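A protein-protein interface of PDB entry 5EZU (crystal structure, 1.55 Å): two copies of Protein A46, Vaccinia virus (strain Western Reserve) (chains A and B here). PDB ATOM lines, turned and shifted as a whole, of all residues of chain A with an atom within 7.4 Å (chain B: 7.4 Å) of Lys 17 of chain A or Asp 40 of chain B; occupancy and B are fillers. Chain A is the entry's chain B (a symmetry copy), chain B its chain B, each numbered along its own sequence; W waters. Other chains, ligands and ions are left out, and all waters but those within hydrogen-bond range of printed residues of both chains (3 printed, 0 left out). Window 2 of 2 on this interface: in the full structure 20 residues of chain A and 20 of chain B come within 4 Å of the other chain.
Water W2 lies within hydrogen-bond range of O of Asp 40 of chain B (2.6 Å), OG of Ser 12 of chain A (2.8 Å) and NE2 of His 42 of chain B (3.2 Å).
Water W1 lies within hydrogen-bond range of OG1 of Thr 41 of chain B, N of Asn 14 of chain A, O of Asp 40 of chain B and NZ of Lys 17 of chain A.
Water W3 bridges the side-chain hydroxyl of Thr 41 of chain A and the side-chain amino group of Lys 17 of chain B.
OD1 of Asn 14 of chain A lies within hydrogen-bond range of N of Ser 16 of chain A (2.9 Å).
The backbone carbonyl oxygen (O) of Val 13 of chain A lies within hydrogen-bond range of the backbone NH (N) of Ile 66 of chain A.
Printed residues of chain B within 4 Å of Val 13 of chain A: Asp 40 (3.9 Å) and Thr 41 (3.6 Å).
Lys 17 of chain A touches just one residue of chain B: Asp 40.
Asp 40 of chain B touches just these residues of chain A: Ser 12, Val 13, Asn 14 and Lys 17.
Printed residues of chain A within 4 Å of Thr 41 of chain B: Ser 12 (3.3 Å) and Val 13 (3.6 Å).
The nearest printed residue of chain B that does not touch Asn 14 of chain A is Thr 41 of chain B (5.1 Å).
O of Ser 12 of chain A lies within hydrogen-bond range of N of His 42 of chain B, at 2.9 Å.
The side-chain amino group (NZ) of Lys 17 of chain A lies within salt-bridge range of the side-chain carboxylate (OD1) of Asp 40 of chain B (2.8 Å).
Hydrophobic or aromatic side chains of chain B that line the printed part of chain A: His 42.
Hydrophobic or aromatic side chains of chain A that line the printed part of chain B: Val 13.
Among the printed residues, 7 pairs touch across the chains.
Among the printed residues, Asp or Glu carboxylates within 4 Å of a Lys or Arg side-chain nitrogen of the other chain: Lys 17 of chain A with Asp 40 of chain B (2.8 Å).
Ser 12 of chain A touches Asp 40 of chain B.
CA of Thr 41 of chain B touches O of Ser 12 of chain A, 3.3 Å away.
Val 13 of chain A touches Asp 40 of chain B.
Val 13 of chain A touches Thr 41 of chain B.
N of Asn 14 of chain A touches O of Asp 40 of chain B, 3.7 Å away.
4 positions are printed for both chains.
Of the 7 pairs that touch across the chains among the printed residues, none has its exchanged pair printed and touching as well.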
ATOM      1  N   SER A  12      24.281 -24.945 -18.792  1.00  0.00           N
ATOM      2  CA  SER A  12      23.615 -24.411 -19.980  1.00  0.00           C
ATOM      3  C   SER A  12      22.172 -24.175 -19.581  1.00  0.00           C
ATOM      4  O   SER A  12      21.586 -25.061 -18.963  1.00  0.00           O
ATOM      5  CB  SER A  12      23.696 -25.406 -21.148  1.00  0.00           C
ATOM      6  OG  SER A  12      22.967 -24.943 -22.275  1.00  0.00           O
ATOM      7  N   VAL A  13      21.612 -23.007 -19.893  1.00  0.00           N
ATOM      8  CA  VAL A  13      20.211 -22.743 -19.599  1.00  0.00           C
ATOM      9  C   VAL A  13      19.565 -22.099 -20.805  1.00  0.00           C
ATOM     10  O   VAL A  13      20.244 -21.435 -21.584  1.00  0.00           O
ATOM     11  CB  VAL A  13      20.014 -21.842 -18.347  1.00  0.00           C
ATOM     12  CG1 VAL A  13      20.790 -22.372 -17.159  1.00  0.00           C
ATOM     13  CG2 VAL A  13      20.410 -20.416 -18.645  1.00  0.00           C
ATOM     14  N   ASN A  14      18.267 -22.289 -20.968  1.00  0.00           N
ATOM     15  CA  ASN A  14      17.582 -21.594 -22.043  1.00  0.00           C
ATOM     16  C   ASN A  14      17.708 -20.096 -21.844  1.00  0.00           C
ATOM     17  O   ASN A  14      17.597 -19.606 -20.729  1.00  0.00           O
ATOM     18  CB  ASN A  14      16.118 -21.991 -22.115  1.00  0.00           C
ATOM     19  CG  ASN A  14      15.400 -21.240 -23.189  1.00  0.00           C
ATOM     20  OD1 ASN A  14      14.864 -20.167 -22.945  1.00  0.00           O
ATOM     21  ND2 ASN A  14      15.423 -21.775 -24.406  1.00  0.00           N
ATOM     22  N   ALA A  15      17.961 -19.372 -22.929  1.00  0.00           N
ATOM     23  CA  ALA A  15      18.360 -17.967 -22.808  1.00  0.00           C
ATOM     24  C   ALA A  15      17.215 -17.039 -22.405  1.00  0.00           C
ATOM     25  O   ALA A  15      17.417 -15.844 -22.229  1.00  0.00           O
ATOM     26  CB  ALA A  15      18.991 -17.491 -24.105  1.00  0.00           C
ATOM     27  N   SER A  16      16.012 -17.574 -22.255  1.00  0.00           N
ATOM     28  CA  SER A  16      14.926 -16.779 -21.707  1.00  0.00           C
ATOM     29  C   SER A  16      15.037 -16.740 -20.185  1.00  0.00           C
ATOM     30  O   SER A  16      14.332 -15.984 -19.525  1.00  0.00           O
ATOM     31  CB  SER A  16      13.573 -17.338 -22.141  1.00  0.00           C
ATOM     32  OG  SER A  16      13.397 -17.178 -23.540  1.00  0.00           O
ATOM     33  N   LYS A  17      15.938 -17.552 -19.634  1.00  0.00           N
ATOM     34  CA  LYS A  17      16.104 -17.609 -18.186  1.00  0.00           C
ATOM     35  C   LYS A  17      17.306 -16.827 -17.710  1.00  0.00           C
ATOM     36  O   LYS A  17      18.234 -16.561 -18.468  1.00  0.00           O
ATOM     37  CB  LYS A  17      16.213 -19.064 -17.717  1.00  0.00           C
ATOM     38  CG  LYS A  17      14.947 -19.867 -18.000  1.00  0.00           C
ATOM     39  CD  LYS A  17      15.064 -21.320 -17.600  1.00  0.00           C
ATOM     40  CE  LYS A  17      13.789 -22.063 -17.991  1.00  0.00           C
ATOM     41  NZ  LYS A  17      13.825 -23.507 -17.631  1.00  0.00           N
ATOM     42  N   THR A  18      17.280 -16.455 -16.440  1.00  0.00           N
ATOM     43  CA  THR A  18      18.386 -15.704 -15.851  1.00  0.00           C
ATOM     44  C   THR A  18      19.116 -16.583 -14.845  1.00  0.00           C
ATOM     45  O   THR A  18      18.473 -17.279 -14.053  1.00  0.00           O
ATOM     46  CB  THR A  18      17.882 -14.414 -15.177  1.00  0.00           C
ATOM     47  OG1 THR A  18      17.393 -13.518 -16.187  1.00  0.00           O
ATOM     48  CG2 THR A  18      18.995 -13.729 -14.391  1.00  0.00           C
ATOM     49  N   ILE A  19      20.448 -16.596 -14.907  1.00  0.00           N
ATOM     50  CA  ILE A  19      21.251 -17.342 -13.954  1.00  0.00           C
ATOM     51  C   ILE A  19      21.675 -16.420 -12.829  1.00  0.00           C
ATOM     52  O   ILE A  19      22.368 -15.438 -13.064  1.00  0.00           O
ATOM     53  CB  ILE A  19      22.509 -17.957 -14.592  1.00  0.00           C
ATOM     54  CG1 ILE A  19      22.125 -18.813 -15.801  1.00  0.00           C
ATOM     55  CG2 ILE A  19      23.302 -18.754 -13.546  1.00  0.00           C
ATOM     56  CD1 ILE A  19      23.298 -19.528 -16.455  1.00  0.00           C
ATOM     57  N   ASN A  20      21.301 -16.754 -11.604  1.00  0.00           N
ATOM     58  CA  ASN A  20      21.748 -16.005 -10.444  1.00  0.00           C
ATOM     59  C   ASN A  20      23.009 -16.687  -9.895  1.00  0.00           C
ATOM     60  O   ASN A  20      22.938 -17.762  -9.296  1.00  0.00           O
ATOM     61  CB  ASN A  20      20.609 -15.931  -9.424  1.00  0.00           C
ATOM     62  CG  ASN A  20      20.972 -15.173  -8.158  1.00  0.00           C
ATOM     63  OD1 ASN A  20      20.291 -15.318  -7.141  1.00  0.00           O
ATOM     64  ND2 ASN A  20      22.044 -14.395  -8.196  1.00  0.00           N
ATOM     65  N   VAL A  38      18.765 -21.099 -10.913  1.00  0.00           N
ATOM     66  CA  VAL A  38      17.922 -20.902 -12.069  1.00  0.00           C
ATOM     67  C   VAL A  38      16.539 -21.297 -11.590  1.00  0.00           C
ATOM     68  O   VAL A  38      16.240 -22.486 -11.465  1.00  0.00           O
ATOM     69  CB  VAL A  38      18.380 -21.760 -13.266  1.00  0.00           C
ATOM     70  CG1 VAL A  38      17.461 -21.547 -14.456  1.00  0.00           C
ATOM     71  CG2 VAL A  38      19.826 -21.460 -13.628  1.00  0.00           C
ATOM     72  N   ASN A  39      15.712 -20.301 -11.276  1.00  0.00           N
ATOM     73  CA  ASN A  39      14.434 -20.535 -10.616  1.00  0.00           C
ATOM     74  C   ASN A  39      14.613 -21.415  -9.379  1.00  0.00           C
ATOM     75  O   ASN A  39      15.389 -21.090  -8.484  1.00  0.00           O
ATOM     76  CB  ASN A  39      13.436 -21.171 -11.583  1.00  0.00           C
ATOM     77  CG  ASN A  39      12.995 -20.215 -12.672  1.00  0.00           C
ATOM     78  OD1 ASN A  39      13.043 -18.998 -12.501  1.00  0.00           O
ATOM     79  ND2 ASN A  39      12.562 -20.766 -13.803  1.00  0.00           N
ATOM     80  N   THR A  41      15.931 -24.323  -9.221  1.00  0.00           N
ATOM     81  CA  THR A  41      17.025 -25.278  -9.335  1.00  0.00           C
ATOM     82  C   THR A  41      18.311 -24.581  -8.926  1.00  0.00           C
ATOM     83  O   THR A  41      18.538 -23.423  -9.312  1.00  0.00           O
ATOM     84  CB  THR A  41      17.174 -25.821 -10.759  1.00  0.00           C
ATOM     85  OG1 THR A  41      15.929 -26.360 -11.193  1.00  0.00           O
ATOM     86  CG2 THR A  41      18.222 -26.917 -10.802  1.00  0.00           C
ATOM     87  N   ASP A  64      20.106 -21.178 -28.625  1.00  0.00           N
ATOM     88  CA  ASP A  64      19.485 -20.102 -27.822  1.00  0.00           C
ATOM     89  C   ASP A  64      19.638 -20.382 -26.337  1.00  0.00           C
ATOM     90  O   ASP A  64      18.652 -20.429 -25.592  1.00  0.00           O
ATOM     91  CB  ASP A  64      18.001 -19.932 -28.197  1.00  0.00           C
ATOM     92  CG  ASP A  64      17.362 -18.664 -27.607  1.00  0.00           C
ATOM     93  OD1 ASP A  64      18.035 -17.612 -27.534  1.00  0.00           O
ATOM     94  OD2 ASP A  64      16.159 -18.718 -27.247  1.00  0.00           O
ATOM     95  N   THR A  65      20.889 -20.585 -25.930  1.00  0.00           N
ATOM     96  CA  THR A  65      21.212 -20.912 -24.549  1.00  0.00           C
ATOM     97  C   THR A  65      22.314 -19.985 -24.036  1.00  0.00           C
ATOM     98  O   THR A  65      23.172 -19.539 -24.804  1.00  0.00           O
ATOM     99  CB  THR A  65      21.700 -22.380 -24.385  1.00  0.00           C
ATOM    100  OG1 THR A  65      22.803 -22.601 -25.270  1.00  0.00           O
ATOM    101  CG2 THR A  65      20.590 -23.374 -24.687  1.00  0.00           C
ATOM    102  N   ILE A  66      22.278 -19.715 -22.738  1.00  0.00           N
ATOM    103  CA  ILE A  66      23.383 -19.092 -22.021  1.00  0.00           C
ATOM    104  C   ILE A  66      24.218 -20.227 -21.456  1.00  0.00           C
ATOM    105  O   ILE A  66      23.673 -21.181 -20.869  1.00  0.00           O
ATOM    106  CB  ILE A  66      22.910 -18.184 -20.895  1.00  0.00           C
ATOM    107  CG1 ILE A  66      22.153 -16.991 -21.432  1.00  0.00           C
ATOM    108  CG2 ILE A  66      24.102 -17.663 -20.058  1.00  0.00           C
ATOM    109  CD1 ILE A  66      21.298 -16.319 -20.370  1.00  0.00           C
ATOM    110  N   LYS B  17      10.055 -32.134 -10.235  1.00  0.00           N
ATOM    111  CA  LYS B  17      10.875 -32.310 -11.428  1.00  0.00           C
ATOM    112  C   LYS B  17      11.702 -33.574 -11.380  1.00  0.00           C
ATOM    113  O   LYS B  17      11.967 -34.122 -10.314  1.00  0.00           O
ATOM    114  CB  LYS B  17      11.790 -31.098 -11.633  1.00  0.00           C
ATOM    115  CG  LYS B  17      11.010 -29.810 -11.879  1.00  0.00           C
ATOM    116  CD  LYS B  17      11.898 -28.595 -12.018  1.00  0.00           C
ATOM    117  CE  LYS B  17      11.037 -27.346 -12.179  1.00  0.00           C
ATOM    118  NZ  LYS B  17      11.839 -26.101 -12.323  1.00  0.00           N
ATOM    119  N   GLU B  37      20.528 -33.231 -16.224  1.00  0.00           N
ATOM    120  CA  GLU B  37      19.624 -32.407 -17.016  1.00  0.00           C
ATOM    121  C   GLU B  37      18.284 -32.302 -16.308  1.00  0.00           C
ATOM    122  O   GLU B  37      17.721 -33.302 -15.862  1.00  0.00           O
ATOM    123  CB  GLU B  37      19.425 -33.015 -18.401  1.00  0.00           C
ATOM    124  CG  GLU B  37      20.710 -33.294 -19.143  1.00  0.00           C
ATOM    125  CD  GLU B  37      20.460 -33.718 -20.574  1.00  0.00           C
ATOM    126  OE1 GLU B  37      19.296 -34.043 -20.902  1.00  0.00           O
ATOM    127  OE2 GLU B  37      21.422 -33.724 -21.372  1.00  0.00           O
ATOM    128  N   VAL B  38      17.772 -31.086 -16.232  1.00  0.00           N
ATOM    129  CA  VAL B  38      16.498 -30.780 -15.623  1.00  0.00           C
ATOM    130  C   VAL B  38      15.805 -29.894 -16.639  1.00  0.00           C
ATOM    131  O   VAL B  38      16.131 -28.711 -16.756  1.00  0.00           O
ATOM    132  CB  VAL B  38      16.668 -30.071 -14.264  1.00  0.00           C
ATOM    133  CG1 VAL B  38      15.313 -29.746 -13.662  1.00  0.00           C
ATOM    134  CG2 VAL B  38      17.504 -30.912 -13.313  1.00  0.00           C
ATOM    135  N   ASN B  39      14.883 -30.475 -17.404  1.00  0.00           N
ATOM    136  CA  ASN B  39      14.287 -29.797 -18.548  1.00  0.00           C
ATOM    137  C   ASN B  39      15.368 -29.215 -19.460  1.00  0.00           C
ATOM    138  O   ASN B  39      16.248 -29.933 -19.927  1.00  0.00           O
ATOM    139  CB  ASN B  39      13.332 -28.699 -18.086  1.00  0.00           C
ATOM    140  CG  ASN B  39      12.082 -29.253 -17.433  1.00  0.00           C
ATOM    141  OD1 ASN B  39      11.685 -30.388 -17.694  1.00  0.00           O
ATOM    142  ND2 ASN B  39      11.456 -28.452 -16.576  1.00  0.00           N
ATOM    143  N   ASP B  40      15.314 -27.907 -19.684  1.00  0.00           N
ATOM    144  CA  ASP B  40      16.230 -27.267 -20.617  1.00  0.00           C
ATOM    145  C   ASP B  40      17.483 -26.756 -19.918  1.00  0.00           C
ATOM    146  O   ASP B  40      18.256 -25.992 -20.496  1.00  0.00           O
ATOM    147  CB  ASP B  40      15.536 -26.112 -21.344  1.00  0.00           C
ATOM    148  CG  ASP B  40      14.479 -25.440 -20.494  1.00  0.00           C
ATOM    149  OD1 ASP B  40      14.436 -25.716 -19.276  1.00  0.00           O
ATOM    150  OD2 ASP B  40      13.696 -24.630 -21.041  1.00  0.00           O
ATOM    151  N   THR B  41      17.697 -27.173 -18.676  1.00  0.00           N
ATOM    152  CA  THR B  41      18.903 -26.762 -17.968  1.00  0.00           C
ATOM    153  C   THR B  41      19.801 -27.977 -17.813  1.00  0.00           C
ATOM    154  O   THR B  41      19.313 -29.073 -17.495  1.00  0.00           O
ATOM    155  CB  THR B  41      18.593 -26.181 -16.586  1.00  0.00           C
ATOM    156  OG1 THR B  41      17.649 -25.123 -16.717  1.00  0.00           O
ATOM    157  CG2 THR B  41      19.855 -25.633 -15.946  1.00  0.00           C
ATOM    158  N   HIS B  42      21.100 -27.807 -18.039  1.00  0.00           N
ATOM    159  CA  HIS B  42      22.056 -28.894 -17.870  1.00  0.00           C
ATOM    160  C   HIS B  42      23.179 -28.431 -16.964  1.00  0.00           C
ATOM    161  O   HIS B  42      23.641 -27.282 -17.059  1.00  0.00           O
ATOM    162  CB  HIS B  42      22.646 -29.353 -19.207  1.00  0.00           C
ATOM    163  CG  HIS B  42      21.680 -29.307 -20.352  1.00  0.00           C
ATOM    164  ND1 HIS B  42      20.698 -30.254 -20.538  1.00  0.00           N
ATOM    165  CD2 HIS B  42      21.558 -28.430 -21.375  1.00  0.00           C
ATOM    166  CE1 HIS B  42      20.006 -29.960 -21.627  1.00  0.00           C
ATOM    167  NE2 HIS B  42      20.508 -28.859 -22.152  1.00  0.00           N
HETATM  168  O   HOH W   1      16.825 -23.834 -18.898  1.00  0.00           O
HETATM  169  O   HOH W   2      20.239 -25.711 -22.117  1.00  0.00           O
HETATM  170  O   HOH W   3      13.738 -26.935  -9.790  1.00  0.00           O
